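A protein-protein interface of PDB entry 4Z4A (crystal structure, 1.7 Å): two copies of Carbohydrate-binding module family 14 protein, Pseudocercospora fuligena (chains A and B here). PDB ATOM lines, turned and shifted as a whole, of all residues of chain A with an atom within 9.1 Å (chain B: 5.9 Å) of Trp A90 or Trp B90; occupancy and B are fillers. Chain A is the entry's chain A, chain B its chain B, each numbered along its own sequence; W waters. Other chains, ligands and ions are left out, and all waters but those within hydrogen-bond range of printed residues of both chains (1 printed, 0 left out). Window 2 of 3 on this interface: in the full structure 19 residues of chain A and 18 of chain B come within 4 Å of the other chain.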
ATOM      1  N   CYS A  52      15.749  16.292  14.221  1.00  0.00           N
ATOM      2  CA  CYS A  52      15.195  17.340  15.097  1.00  0.00           C
ATOM      3  C   CYS A  52      13.830  17.899  14.646  1.00  0.00           C
ATOM      4  O   CYS A  52      13.073  18.425  15.462  1.00  0.00           O
ATOM      5  CB  CYS A  52      16.212  18.487  15.205  1.00  0.00           C
ATOM      6  SG  CYS A  52      17.785  17.825  15.810  1.00  0.00           S
ATOM      7  N   ASN A  53      13.511  17.789  13.360  1.00  0.00           N
ATOM      8  CA  ASN A  53      12.277  18.284  12.757  1.00  0.00           C
ATOM      9  C   ASN A  53      11.183  17.151  12.829  1.00  0.00           C
ATOM     10  O   ASN A  53      10.500  16.883  11.840  1.00  0.00           O
ATOM     11  CB  ASN A  53      12.537  18.562  11.288  1.00  0.00           C
ATOM     12  CG  ASN A  53      11.355  19.151  10.513  1.00  0.00           C
ATOM     13  OD1 ASN A  53      11.129  18.717   9.364  1.00  0.00           O
ATOM     14  ND2 ASN A  53      10.631  20.118  11.073  1.00  0.00           N
ATOM     15  N   CYS A  75       7.587  17.332  12.426  1.00  0.00           N
ATOM     16  CA  CYS A  75       7.208  18.707  12.802  1.00  0.00           C
ATOM     17  C   CYS A  75       6.928  19.537  11.542  1.00  0.00           C
ATOM     18  O   CYS A  75       7.437  19.243  10.417  1.00  0.00           O
ATOM     19  CB  CYS A  75       8.305  19.322  13.661  1.00  0.00           C
ATOM     20  SG  CYS A  75       8.424  18.594  15.360  1.00  0.00           S
ATOM     21  N   PRO A  76       6.178  20.609  11.710  1.00  0.00           N
ATOM     22  CA  PRO A  76       5.994  21.539  10.601  1.00  0.00           C
ATOM     23  C   PRO A  76       7.320  22.202  10.126  1.00  0.00           C
ATOM     24  O   PRO A  76       8.337  22.160  10.821  1.00  0.00           O
ATOM     25  CB  PRO A  76       5.081  22.623  11.197  1.00  0.00           C
ATOM     26  CG  PRO A  76       4.344  21.904  12.324  1.00  0.00           C
ATOM     27  CD  PRO A  76       5.413  21.024  12.917  1.00  0.00           C
ATOM     28  N   SER A  77       7.270  22.744   8.923  1.00  0.00           N
ATOM     29  CA  SER A  77       8.479  23.230   8.252  1.00  0.00           C
ATOM     30  C   SER A  77       9.239  24.162   9.152  1.00  0.00           C
ATOM     31  O   SER A  77       8.651  25.104   9.674  1.00  0.00           O
ATOM     32  CB  SER A  77       8.070  23.978   6.975  1.00  0.00           C
ATOM     33  OG  SER A  77       7.641  22.993   6.079  1.00  0.00           O
ATOM     34  N   GLY A  78      10.543  23.907   9.332  1.00  0.00           N
ATOM     35  CA  GLY A  78      11.396  24.801  10.138  1.00  0.00           C
ATOM     36  C   GLY A  78      11.332  24.585  11.643  1.00  0.00           C
ATOM     37  O   GLY A  78      12.239  25.006  12.389  1.00  0.00           O
ATOM     38  N   LEU A  79      10.325  23.820  12.127  1.00  0.00           N
ATOM     39  CA  LEU A  79      10.146  23.704  13.582  1.00  0.00           C
ATOM     40  C   LEU A  79      10.873  22.465  14.112  1.00  0.00           C
ATOM     41  O   LEU A  79      11.180  21.538  13.347  1.00  0.00           O
ATOM     42  CB  LEU A  79       8.661  23.654  13.917  1.00  0.00           C
ATOM     43  CG  LEU A  79       7.727  24.763  13.445  1.00  0.00           C
ATOM     44  CD1 LEU A  79       6.375  24.596  14.105  1.00  0.00           C
ATOM     45  CD2 LEU A  79       8.343  26.096  13.763  1.00  0.00           C
ATOM     46  N   LEU A  80      11.193  22.490  15.408  1.00  0.00           N
ATOM     47  CA  LEU A  80      12.010  21.477  16.034  1.00  0.00           C
ATOM     48  C   LEU A  80      11.382  20.988  17.315  1.00  0.00           C
ATOM     49  O   LEU A  80      10.601  21.693  17.960  1.00  0.00           O
ATOM     50  CB  LEU A  80      13.398  22.093  16.393  1.00  0.00           C
ATOM     51  CG  LEU A  80      14.217  22.626  15.247  1.00  0.00           C
ATOM     52  CD1 LEU A  80      15.495  23.233  15.894  1.00  0.00           C
ATOM     53  CD2 LEU A  80      14.516  21.616  14.161  1.00  0.00           C
ATOM     54  N   TRP A  81      11.702  19.733  17.691  1.00  0.00           N
ATOM     55  CA  TRP A  81      11.174  19.194  18.873  1.00  0.00           C
ATOM     56  C   TRP A  81      11.615  19.875  20.128  1.00  0.00           C
ATOM     57  O   TRP A  81      12.804  20.087  20.334  1.00  0.00           O
ATOM     58  CB  TRP A  81      11.574  17.710  18.962  1.00  0.00           C
ATOM     59  CG  TRP A  81      10.881  16.910  20.077  1.00  0.00           C
ATOM     60  CD1 TRP A  81      11.494  16.319  21.142  1.00  0.00           C
ATOM     61  CD2 TRP A  81       9.479  16.705  20.255  1.00  0.00           C
ATOM     62  NE1 TRP A  81      10.568  15.754  21.964  1.00  0.00           N
ATOM     63  CE2 TRP A  81       9.320  15.942  21.428  1.00  0.00           C
ATOM     64  CE3 TRP A  81       8.338  17.082  19.522  1.00  0.00           C
ATOM     65  CZ2 TRP A  81       8.072  15.488  21.882  1.00  0.00           C
ATOM     66  CZ3 TRP A  81       7.091  16.654  19.984  1.00  0.00           C
ATOM     67  CH2 TRP A  81       6.984  15.830  21.149  1.00  0.00           C
ATOM     68  N   ASN A  82      10.660  20.114  21.012  1.00  0.00           N
ATOM     69  CA  ASN A  82      10.925  20.651  22.348  1.00  0.00           C
ATOM     70  C   ASN A  82      10.441  19.639  23.386  1.00  0.00           C
ATOM     71  O   ASN A  82       9.252  19.564  23.730  1.00  0.00           O
ATOM     72  CB  ASN A  82      10.233  22.020  22.493  1.00  0.00           C
ATOM     73  CG  ASN A  82      10.201  22.525  23.934  1.00  0.00           C
ATOM     74  OD1 ASN A  82      10.748  21.917  24.843  1.00  0.00           O
ATOM     75  ND2 ASN A  82       9.596  23.661  24.130  1.00  0.00           N
ATOM     76  N   LYS A  85       8.303  20.609  26.714  1.00  0.00           N
ATOM     77  CA  LYS A  85       6.873  20.774  26.613  1.00  0.00           C
ATOM     78  C   LYS A  85       6.236  19.643  25.785  1.00  0.00           C
ATOM     79  O   LYS A  85       5.009  19.612  25.656  1.00  0.00           O
ATOM     80  CB  LYS A  85       6.530  22.125  25.991  1.00  0.00           C
ATOM     81  CG  LYS A  85       6.857  23.299  26.894  1.00  0.00           C
ATOM     82  CD  LYS A  85       6.192  24.557  26.418  1.00  0.00           C
ATOM     83  CE  LYS A  85       6.467  25.701  27.394  1.00  0.00           C
ATOM     84  NZ  LYS A  85       5.864  26.971  26.864  1.00  0.00           N
ATOM     85  N   TRP A  87       6.301  19.039  22.527  1.00  0.00           N
ATOM     86  CA  TRP A  87       5.647  19.482  21.299  1.00  0.00           C
ATOM     87  C   TRP A  87       6.650  20.029  20.270  1.00  0.00           C
ATOM     88  O   TRP A  87       7.804  20.387  20.614  1.00  0.00           O
ATOM     89  CB  TRP A  87       4.510  20.493  21.601  1.00  0.00           C
ATOM     90  CG  TRP A  87       4.860  21.870  22.084  1.00  0.00           C
ATOM     91  CD1 TRP A  87       6.103  22.377  22.380  1.00  0.00           C
ATOM     92  CD2 TRP A  87       3.937  22.900  22.375  1.00  0.00           C
ATOM     93  NE1 TRP A  87       5.995  23.681  22.778  1.00  0.00           N
ATOM     94  CE2 TRP A  87       4.674  24.016  22.791  1.00  0.00           C
ATOM     95  CE3 TRP A  87       2.546  23.013  22.261  1.00  0.00           C
ATOM     96  CZ2 TRP A  87       4.072  25.220  23.107  1.00  0.00           C
ATOM     97  CZ3 TRP A  87       1.956  24.211  22.586  1.00  0.00           C
ATOM     98  CH2 TRP A  87       2.717  25.296  22.982  1.00  0.00           C
ATOM     99  N   CYS A  88       6.158  20.122  19.035  1.00  0.00           N
ATOM    100  CA  CYS A  88       6.852  20.808  17.967  1.00  0.00           C
ATOM    101  C   CYS A  88       6.799  22.294  18.269  1.00  0.00           C
ATOM    102  O   CYS A  88       5.745  22.780  18.577  1.00  0.00           O
ATOM    103  CB  CYS A  88       6.194  20.542  16.611  1.00  0.00           C
ATOM    104  SG  CYS A  88       6.360  18.776  16.148  1.00  0.00           S
ATOM    105  N   ASP A  89       7.927  22.988  18.199  1.00  0.00           N
ATOM    106  CA  ASP A  89       8.015  24.377  18.672  1.00  0.00           C
ATOM    107  C   ASP A  89       8.982  25.190  17.842  1.00  0.00           C
ATOM    108  O   ASP A  89       9.757  24.638  17.036  1.00  0.00           O
ATOM    109  CB  ASP A  89       8.474  24.372  20.159  1.00  0.00           C
ATOM    110  CG  ASP A  89       8.043  25.616  20.973  1.00  0.00           C
ATOM    111  OD1 ASP A  89       7.603  26.668  20.434  1.00  0.00           O
ATOM    112  OD2 ASP A  89       8.208  25.501  22.221  1.00  0.00           O
ATOM    113  N   TRP A  90       8.958  26.501  18.066  1.00  0.00           N
ATOM    114  CA  TRP A  90       9.920  27.363  17.454  1.00  0.00           C
ATOM    115  C   TRP A  90      11.355  26.907  17.740  1.00  0.00           C
ATOM    116  O   TRP A  90      11.652  26.459  18.837  1.00  0.00           O
ATOM    117  CB  TRP A  90       9.669  28.816  17.935  1.00  0.00           C
ATOM    118  CG  TRP A  90       8.309  29.272  17.546  1.00  0.00           C
ATOM    119  CD1 TRP A  90       7.221  29.417  18.359  1.00  0.00           C
ATOM    120  CD2 TRP A  90       7.845  29.527  16.228  1.00  0.00           C
ATOM    121  NE1 TRP A  90       6.133  29.780  17.634  1.00  0.00           N
ATOM    122  CE2 TRP A  90       6.479  29.838  16.319  1.00  0.00           C
ATOM    123  CE3 TRP A  90       8.445  29.479  14.967  1.00  0.00           C
ATOM    124  CZ2 TRP A  90       5.698  30.145  15.200  1.00  0.00           C
ATOM    125  CZ3 TRP A  90       7.680  29.788  13.845  1.00  0.00           C
ATOM    126  CH2 TRP A  90       6.323  30.132  13.968  1.00  0.00           C
ATOM    127  N   PRO A  91      12.254  26.995  16.730  1.00  0.00           N
ATOM    128  CA  PRO A  91      13.592  26.442  16.943  1.00  0.00           C
ATOM    129  C   PRO A  91      14.324  26.959  18.172  1.00  0.00           C
ATOM    130  O   PRO A  91      15.112  26.199  18.772  1.00  0.00           O
ATOM    131  CB  PRO A  91      14.323  26.722  15.633  1.00  0.00           C
ATOM    132  CG  PRO A  91      13.281  27.114  14.643  1.00  0.00           C
ATOM    133  CD  PRO A  91      12.083  27.587  15.384  1.00  0.00           C
ATOM    134  N   GLU A  92      14.095  28.226  18.591  1.00  0.00           N
ATOM    135  CA  GLU A  92      14.734  28.706  19.818  1.00  0.00           C
ATOM    136  C   GLU A  92      14.456  27.915  21.096  1.00  0.00           C
ATOM    137  O   GLU A  92      15.266  27.927  22.029  1.00  0.00           O
ATOM    138  CB  GLU A  92      14.384  30.205  20.083  1.00  0.00           C
ATOM    139  CG  GLU A  92      12.936  30.468  20.471  1.00  0.00           C
ATOM    140  CD  GLU A  92      12.588  31.937  20.348  1.00  0.00           C
ATOM    141  OE1 GLU A  92      12.456  32.560  21.418  1.00  0.00           O
ATOM    142  OE2 GLU A  92      12.439  32.430  19.193  1.00  0.00           O
ATOM    143  N   ASN A  93      13.351  27.126  21.097  1.00  0.00           N
ATOM    144  CA  ASN A  93      12.965  26.385  22.283  1.00  0.00           C
ATOM    145  C   ASN A  93      13.319  24.902  22.215  1.00  0.00           C
ATOM    146  O   ASN A  93      12.905  24.168  23.076  1.00  0.00           O
ATOM    147  CB  ASN A  93      11.468  26.509  22.508  1.00  0.00           C
ATOM    148  CG  ASN A  93      11.041  27.921  22.787  1.00  0.00           C
ATOM    149  OD1 ASN A  93      11.797  28.664  23.386  1.00  0.00           O
ATOM    150  ND2 ASN A  93       9.857  28.298  22.335  1.00  0.00           N
ATOM    151  N   THR A  94      14.124  24.499  21.238  1.00  0.00           N
ATOM    152  CA  THR A  94      14.462  23.090  21.024  1.00  0.00           C
ATOM    153  C   THR A  94      15.297  22.471  22.132  1.00  0.00           C
ATOM    154  O   THR A  94      16.078  23.161  22.834  1.00  0.00           O
ATOM    155  CB  THR A  94      15.119  22.887  19.627  1.00  0.00           C
ATOM    156  OG1 THR A  94      15.111  21.494  19.254  1.00  0.00           O
ATOM    157  CG2 THR A  94      16.574  23.269  19.604  1.00  0.00           C
ATOM    158  N   THR A  95      15.127  21.166  22.260  1.00  0.00           N
ATOM    159  CA  THR A  95      16.000  20.325  23.076  1.00  0.00           C
ATOM    160  C   THR A  95      16.911  19.469  22.213  1.00  0.00           C
ATOM    161  O   THR A  95      17.688  18.678  22.747  1.00  0.00           O
ATOM    162  CB  THR A  95      15.165  19.471  24.007  1.00  0.00           C
ATOM    163  OG1 THR A  95      14.145  18.803  23.222  1.00  0.00           O
ATOM    164  CG2 THR A  95      14.511  20.322  25.053  1.00  0.00           C
ATOM    165  N   CYS A  96      16.848  19.644  20.891  1.00  0.00           N
ATOM    166  CA  CYS A  96      17.591  18.766  20.010  1.00  0.00           C
ATOM    167  C   CYS A  96      19.103  18.835  20.241  1.00  0.00           C
ATOM    168  O   CYS A  96      19.687  19.898  20.380  1.00  0.00           O
ATOM    169  CB  CYS A  96      17.236  18.950  18.533  1.00  0.00           C
ATOM    170  SG  CYS A  96      17.302  17.371  17.623  1.00  0.00           S
ATOM    171  N   PRO B  76       1.453  26.263  19.767  1.00  0.00           N
ATOM    172  CA  PRO B  76       2.505  27.244  19.992  1.00  0.00           C
ATOM    173  C   PRO B  76       2.063  28.631  19.481  1.00  0.00           C
ATOM    174  O   PRO B  76       1.312  28.764  18.494  1.00  0.00           O
ATOM    175  CB  PRO B  76       3.698  26.683  19.209  1.00  0.00           C
ATOM    176  CG  PRO B  76       3.444  25.201  19.234  1.00  0.00           C
ATOM    177  CD  PRO B  76       1.965  25.058  19.091  1.00  0.00           C
ATOM    178  N   SER B  77       2.515  29.685  20.132  1.00  0.00           N
ATOM    179  CA  SER B  77       2.255  31.056  19.669  1.00  0.00           C
ATOM    180  C   SER B  77       2.507  31.194  18.176  1.00  0.00           C
ATOM    181  O   SER B  77       3.568  30.838  17.682  1.00  0.00           O
ATOM    182  CB  SER B  77       3.169  32.036  20.421  1.00  0.00           C
ATOM    183  OG  SER B  77       2.940  33.400  20.034  1.00  0.00           O
ATOM    184  N   GLY B  78       1.546  31.722  17.449  1.00  0.00           N
ATOM    185  CA  GLY B  78       1.736  31.973  16.043  1.00  0.00           C
ATOM    186  C   GLY B  78       1.344  30.843  15.109  1.00  0.00           C
ATOM    187  O   GLY B  78       1.443  31.009  13.890  1.00  0.00           O
ATOM    188  N   LEU B  79       1.001  29.683  15.671  1.00  0.00           N
ATOM    189  CA  LEU B  79       0.557  28.534  14.879  1.00  0.00           C
ATOM    190  C   LEU B  79      -0.935  28.375  15.063  1.00  0.00           C
ATOM    191  O   LEU B  79      -1.492  28.750  16.103  1.00  0.00           O
ATOM    192  CB  LEU B  79       1.308  27.278  15.314  1.00  0.00           C
ATOM    193  CG  LEU B  79       2.833  27.296  15.228  1.00  0.00           C
ATOM    194  CD1 LEU B  79       3.404  25.916  15.569  1.00  0.00           C
ATOM    195  CD2 LEU B  79       3.284  27.733  13.844  1.00  0.00           C
ATOM    196  N   LEU B  80      -1.574  27.845  14.032  1.00  0.00           N
ATOM    197  CA  LEU B  80      -3.000  27.670  13.983  1.00  0.00           C
ATOM    198  C   LEU B  80      -3.272  26.198  13.668  1.00  0.00           C
ATOM    199  O   LEU B  80      -2.482  25.532  13.018  1.00  0.00           O
ATOM    200  CB  LEU B  80      -3.625  28.537  12.889  1.00  0.00           C
ATOM    201  CG  LEU B  80      -3.449  30.058  13.047  1.00  0.00           C
ATOM    202  CD1 LEU B  80      -4.200  30.715  11.919  1.00  0.00           C
ATOM    203  CD2 LEU B  80      -3.844  30.584  14.430  1.00  0.00           C
ATOM    204  N   CYS B  88      -0.858  21.457  14.731  1.00  0.00           N
ATOM    205  CA  CYS B  88      -0.586  22.921  14.775  1.00  0.00           C
ATOM    206  C   CYS B  88       0.398  23.266  13.660  1.00  0.00           C
ATOM    207  O   CYS B  88       1.385  22.583  13.470  1.00  0.00           O
ATOM    208  CB  CYS B  88      -0.037  23.310  16.145  1.00  0.00           C
ATOM    209  SG  CYS B  88      -1.207  23.012  17.474  1.00  0.00           S
ATOM    210  N   ASP B  89       0.124  24.316  12.891  1.00  0.00           N
ATOM    211  CA  ASP B  89       0.862  24.536  11.654  1.00  0.00           C
ATOM    212  C   ASP B  89       0.907  26.062  11.381  1.00  0.00           C
ATOM    213  O   ASP B  89       0.253  26.861  12.052  1.00  0.00           O
ATOM    214  CB  ASP B  89       0.203  23.721  10.529  1.00  0.00           C
ATOM    215  CG  ASP B  89       1.055  23.503   9.264  1.00  0.00           C
ATOM    216  OD1 ASP B  89       2.230  23.890   9.137  1.00  0.00           O
ATOM    217  OD2 ASP B  89       0.558  22.795   8.355  1.00  0.00           O
ATOM    218  N   TRP B  90       1.756  26.393  10.416  1.00  0.00           N
ATOM    219  CA  TRP B  90       1.889  27.794   9.959  1.00  0.00           C
ATOM    220  C   TRP B  90       0.496  28.296   9.603  1.00  0.00           C
ATOM    221  O   TRP B  90      -0.313  27.567   9.012  1.00  0.00           O
ATOM    222  CB  TRP B  90       2.826  27.842   8.762  1.00  0.00           C
ATOM    223  CG  TRP B  90       4.236  27.536   9.121  1.00  0.00           C
ATOM    224  CD1 TRP B  90       4.855  26.350   9.114  1.00  0.00           C
ATOM    225  CD2 TRP B  90       5.219  28.496   9.550  1.00  0.00           C
ATOM    226  NE1 TRP B  90       6.171  26.466   9.526  1.00  0.00           N
ATOM    227  CE2 TRP B  90       6.423  27.786   9.777  1.00  0.00           C
ATOM    228  CE3 TRP B  90       5.195  29.886   9.732  1.00  0.00           C
ATOM    229  CZ2 TRP B  90       7.586  28.414  10.221  1.00  0.00           C
ATOM    230  CZ3 TRP B  90       6.371  30.517  10.144  1.00  0.00           C
ATOM    231  CH2 TRP B  90       7.538  29.789  10.371  1.00  0.00           C
ATOM    232  N   PRO B  91       0.195  29.537   9.940  1.00  0.00           N
ATOM    233  CA  PRO B  91      -1.126  30.129   9.683  1.00  0.00           C
ATOM    234  C   PRO B  91      -1.639  30.018   8.268  1.00  0.00           C
ATOM    235  O   PRO B  91      -2.849  29.890   8.079  1.00  0.00           O
ATOM    236  CB  PRO B  91      -0.916  31.624  10.001  1.00  0.00           C
ATOM    237  CG  PRO B  91       0.164  31.656  10.965  1.00  0.00           C
ATOM    238  CD  PRO B  91       1.050  30.457  10.724  1.00  0.00           C
ATOM    239  N   GLU B  92      -0.756  30.030   7.285  1.00  0.00           N
ATOM    240  CA  GLU B  92      -1.178  29.971   5.900  1.00  0.00           C
ATOM    241  C   GLU B  92      -1.833  28.645   5.560  1.00  0.00           C
ATOM    242  O   GLU B  92      -2.514  28.539   4.548  1.00  0.00           O
ATOM    243  CB  GLU B  92       0.004  30.193   4.944  1.00  0.00           C
ATOM    244  CG  GLU B  92       1.054  29.092   4.951  1.00  0.00           C
ATOM    245  CD  GLU B  92       2.446  29.495   4.448  1.00  0.00           C
ATOM    246  OE1 GLU B  92       2.985  28.785   3.568  1.00  0.00           O
ATOM    247  OE2 GLU B  92       3.032  30.481   4.958  1.00  0.00           O
ATOM    248  N   ASN B  93      -1.532  27.634   6.378  1.00  0.00           N
ATOM    249  CA  ASN B  93      -2.111  26.314   6.183  1.00  0.00           C
ATOM    250  C   ASN B  93      -3.335  26.004   7.020  1.00  0.00           C
ATOM    251  O   ASN B  93      -3.804  24.820   7.052  1.00  0.00           O
ATOM    252  CB  ASN B  93      -1.044  25.286   6.526  1.00  0.00           C
ATOM    253  CG  ASN B  93       0.162  25.411   5.644  1.00  0.00           C
ATOM    254  OD1 ASN B  93       0.044  25.725   4.446  1.00  0.00           O
ATOM    255  ND2 ASN B  93       1.342  25.160   6.212  1.00  0.00           N
ATOM    256  N   THR B  94      -3.910  26.990   7.675  1.00  0.00           N
ATOM    257  CA  THR B  94      -5.007  26.706   8.599  1.00  0.00           C
ATOM    258  C   THR B  94      -6.300  26.316   7.908  1.00  0.00           C
ATOM    259  O   THR B  94      -6.612  26.772   6.807  1.00  0.00           O
ATOM    260  CB  THR B  94      -5.275  27.881   9.542  1.00  0.00           C
ATOM    261  OG1 THR B  94      -6.071  27.430  10.629  1.00  0.00           O
ATOM    262  CG2 THR B  94      -5.955  29.049   8.813  1.00  0.00           C
HETATM  263  O   HOH W   1       4.539  22.877   7.730  1.00  0.00           O
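Pro A76 touches Cys B88 (CG to O, 3.2 Å).
CB of Pro A76 touches OD1 of Asp B89, at 3.7 Å.
Leu A79 touches Leu B79 (CD1 to CD1, 3.6 Å).
N of Pro B76 touches CZ3 of Trp A87, at 3.5 Å.
O of Cys A88 touches CG of Pro B76, at 3.4 Å.
CD2 of Leu B79 touches CZ2 of Trp A90, at 3.7 Å.
Trp A90 touches Trp B90 (CZ3 to CH2, 3.5 Å).
Of the 21 printed residues of chain A, 6 touch a printed residue of chain B.
Hydrophobic or aromatic side chains of chain A within 4 Å of the printed part of chain B: Pro A76, Leu A79, Trp A87 and Trp A90.
Among the printed residues, 9 pairs touch across the chains.
The side-chain sulfur of Cys A96 is disulfide-bonded to the side-chain sulfur of Cys A52 (1.9 Å).
ND2 of Asn A53 is in hydrogen-bond range of O of Leu A79 (2.7 Å).
The side-chain sulfur of Cys A75 forms a disulfide with the side-chain sulfur of Cys A88 (2.2 Å).
The backbone NH (N) of Asn A82 sits at hydrogen-bond distance from the backbone carbonyl oxygen (O) of Trp A87, 2.9 Å away.
The backbone NH (N) of Leu B80 is in hydrogen-bond range of the backbone carbonyl oxygen (O) of Asp B89 (2.9 Å).
The side-chain carboxylate (OD2) of Asp B89 sits at hydrogen-bond distance from the side-chain amide nitrogen (ND2) of Asn B93, 3.3 Å away.
Water W1 bridges the side-chain carboxylate (OD1) of Asp B89 and the backbone NH (N) of Ser A77.
Pro A76 touches Cys B88, and with the chains exchanged Cys A88 touches Pro B76.
Pro A76 touches Asp B89, but with the chains exchanged Asp A89 does not touch Pro B76 (4.1 Å).
Ser A77 touches Trp B90, and with the chains exchanged Trp A90 touches Ser B77.
Trp A90 touches Leu B79, but with the chains exchanged Leu A79 does not touch Trp B90 (4.3 Å).
Of the printed residues of chain B, Pro A76 touches Cys B88 (3.2 Å) and Asp B89 (3.7 Å).
Printed residues of chain B within 4 Å of Ser A77: Trp B90.
Printed residues of chain B within 4 Å of Trp A90: Ser B77, Leu B79 and Trp B90.
Of the printed residues of chain A, Pro B76 touches Trp A87 and Cys A88.
Printed residues of chain A within 4 Å of Ser B77: Trp A90 (2.8 Å).
No residue of chain A comes within 4 Å of Gly B78.
Of the printed residues of chain A, Leu B79 touches Leu A79 and Trp A90.
Trp B90 touches just these residues of chain A: Ser A77 and Trp A90.
No residue of chain A comes within 4 Å of Pro B91.
The indole nitrogen (NE1) of Trp B90 is in hydrogen-bond range of the backbone carbonyl oxygen (O) of Ser A77 (2.8 Å).
The backbone carbonyl oxygen of Ser B77 is in hydrogen-bond range of the indole nitrogen of Trp A90, 2.8 Å away.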
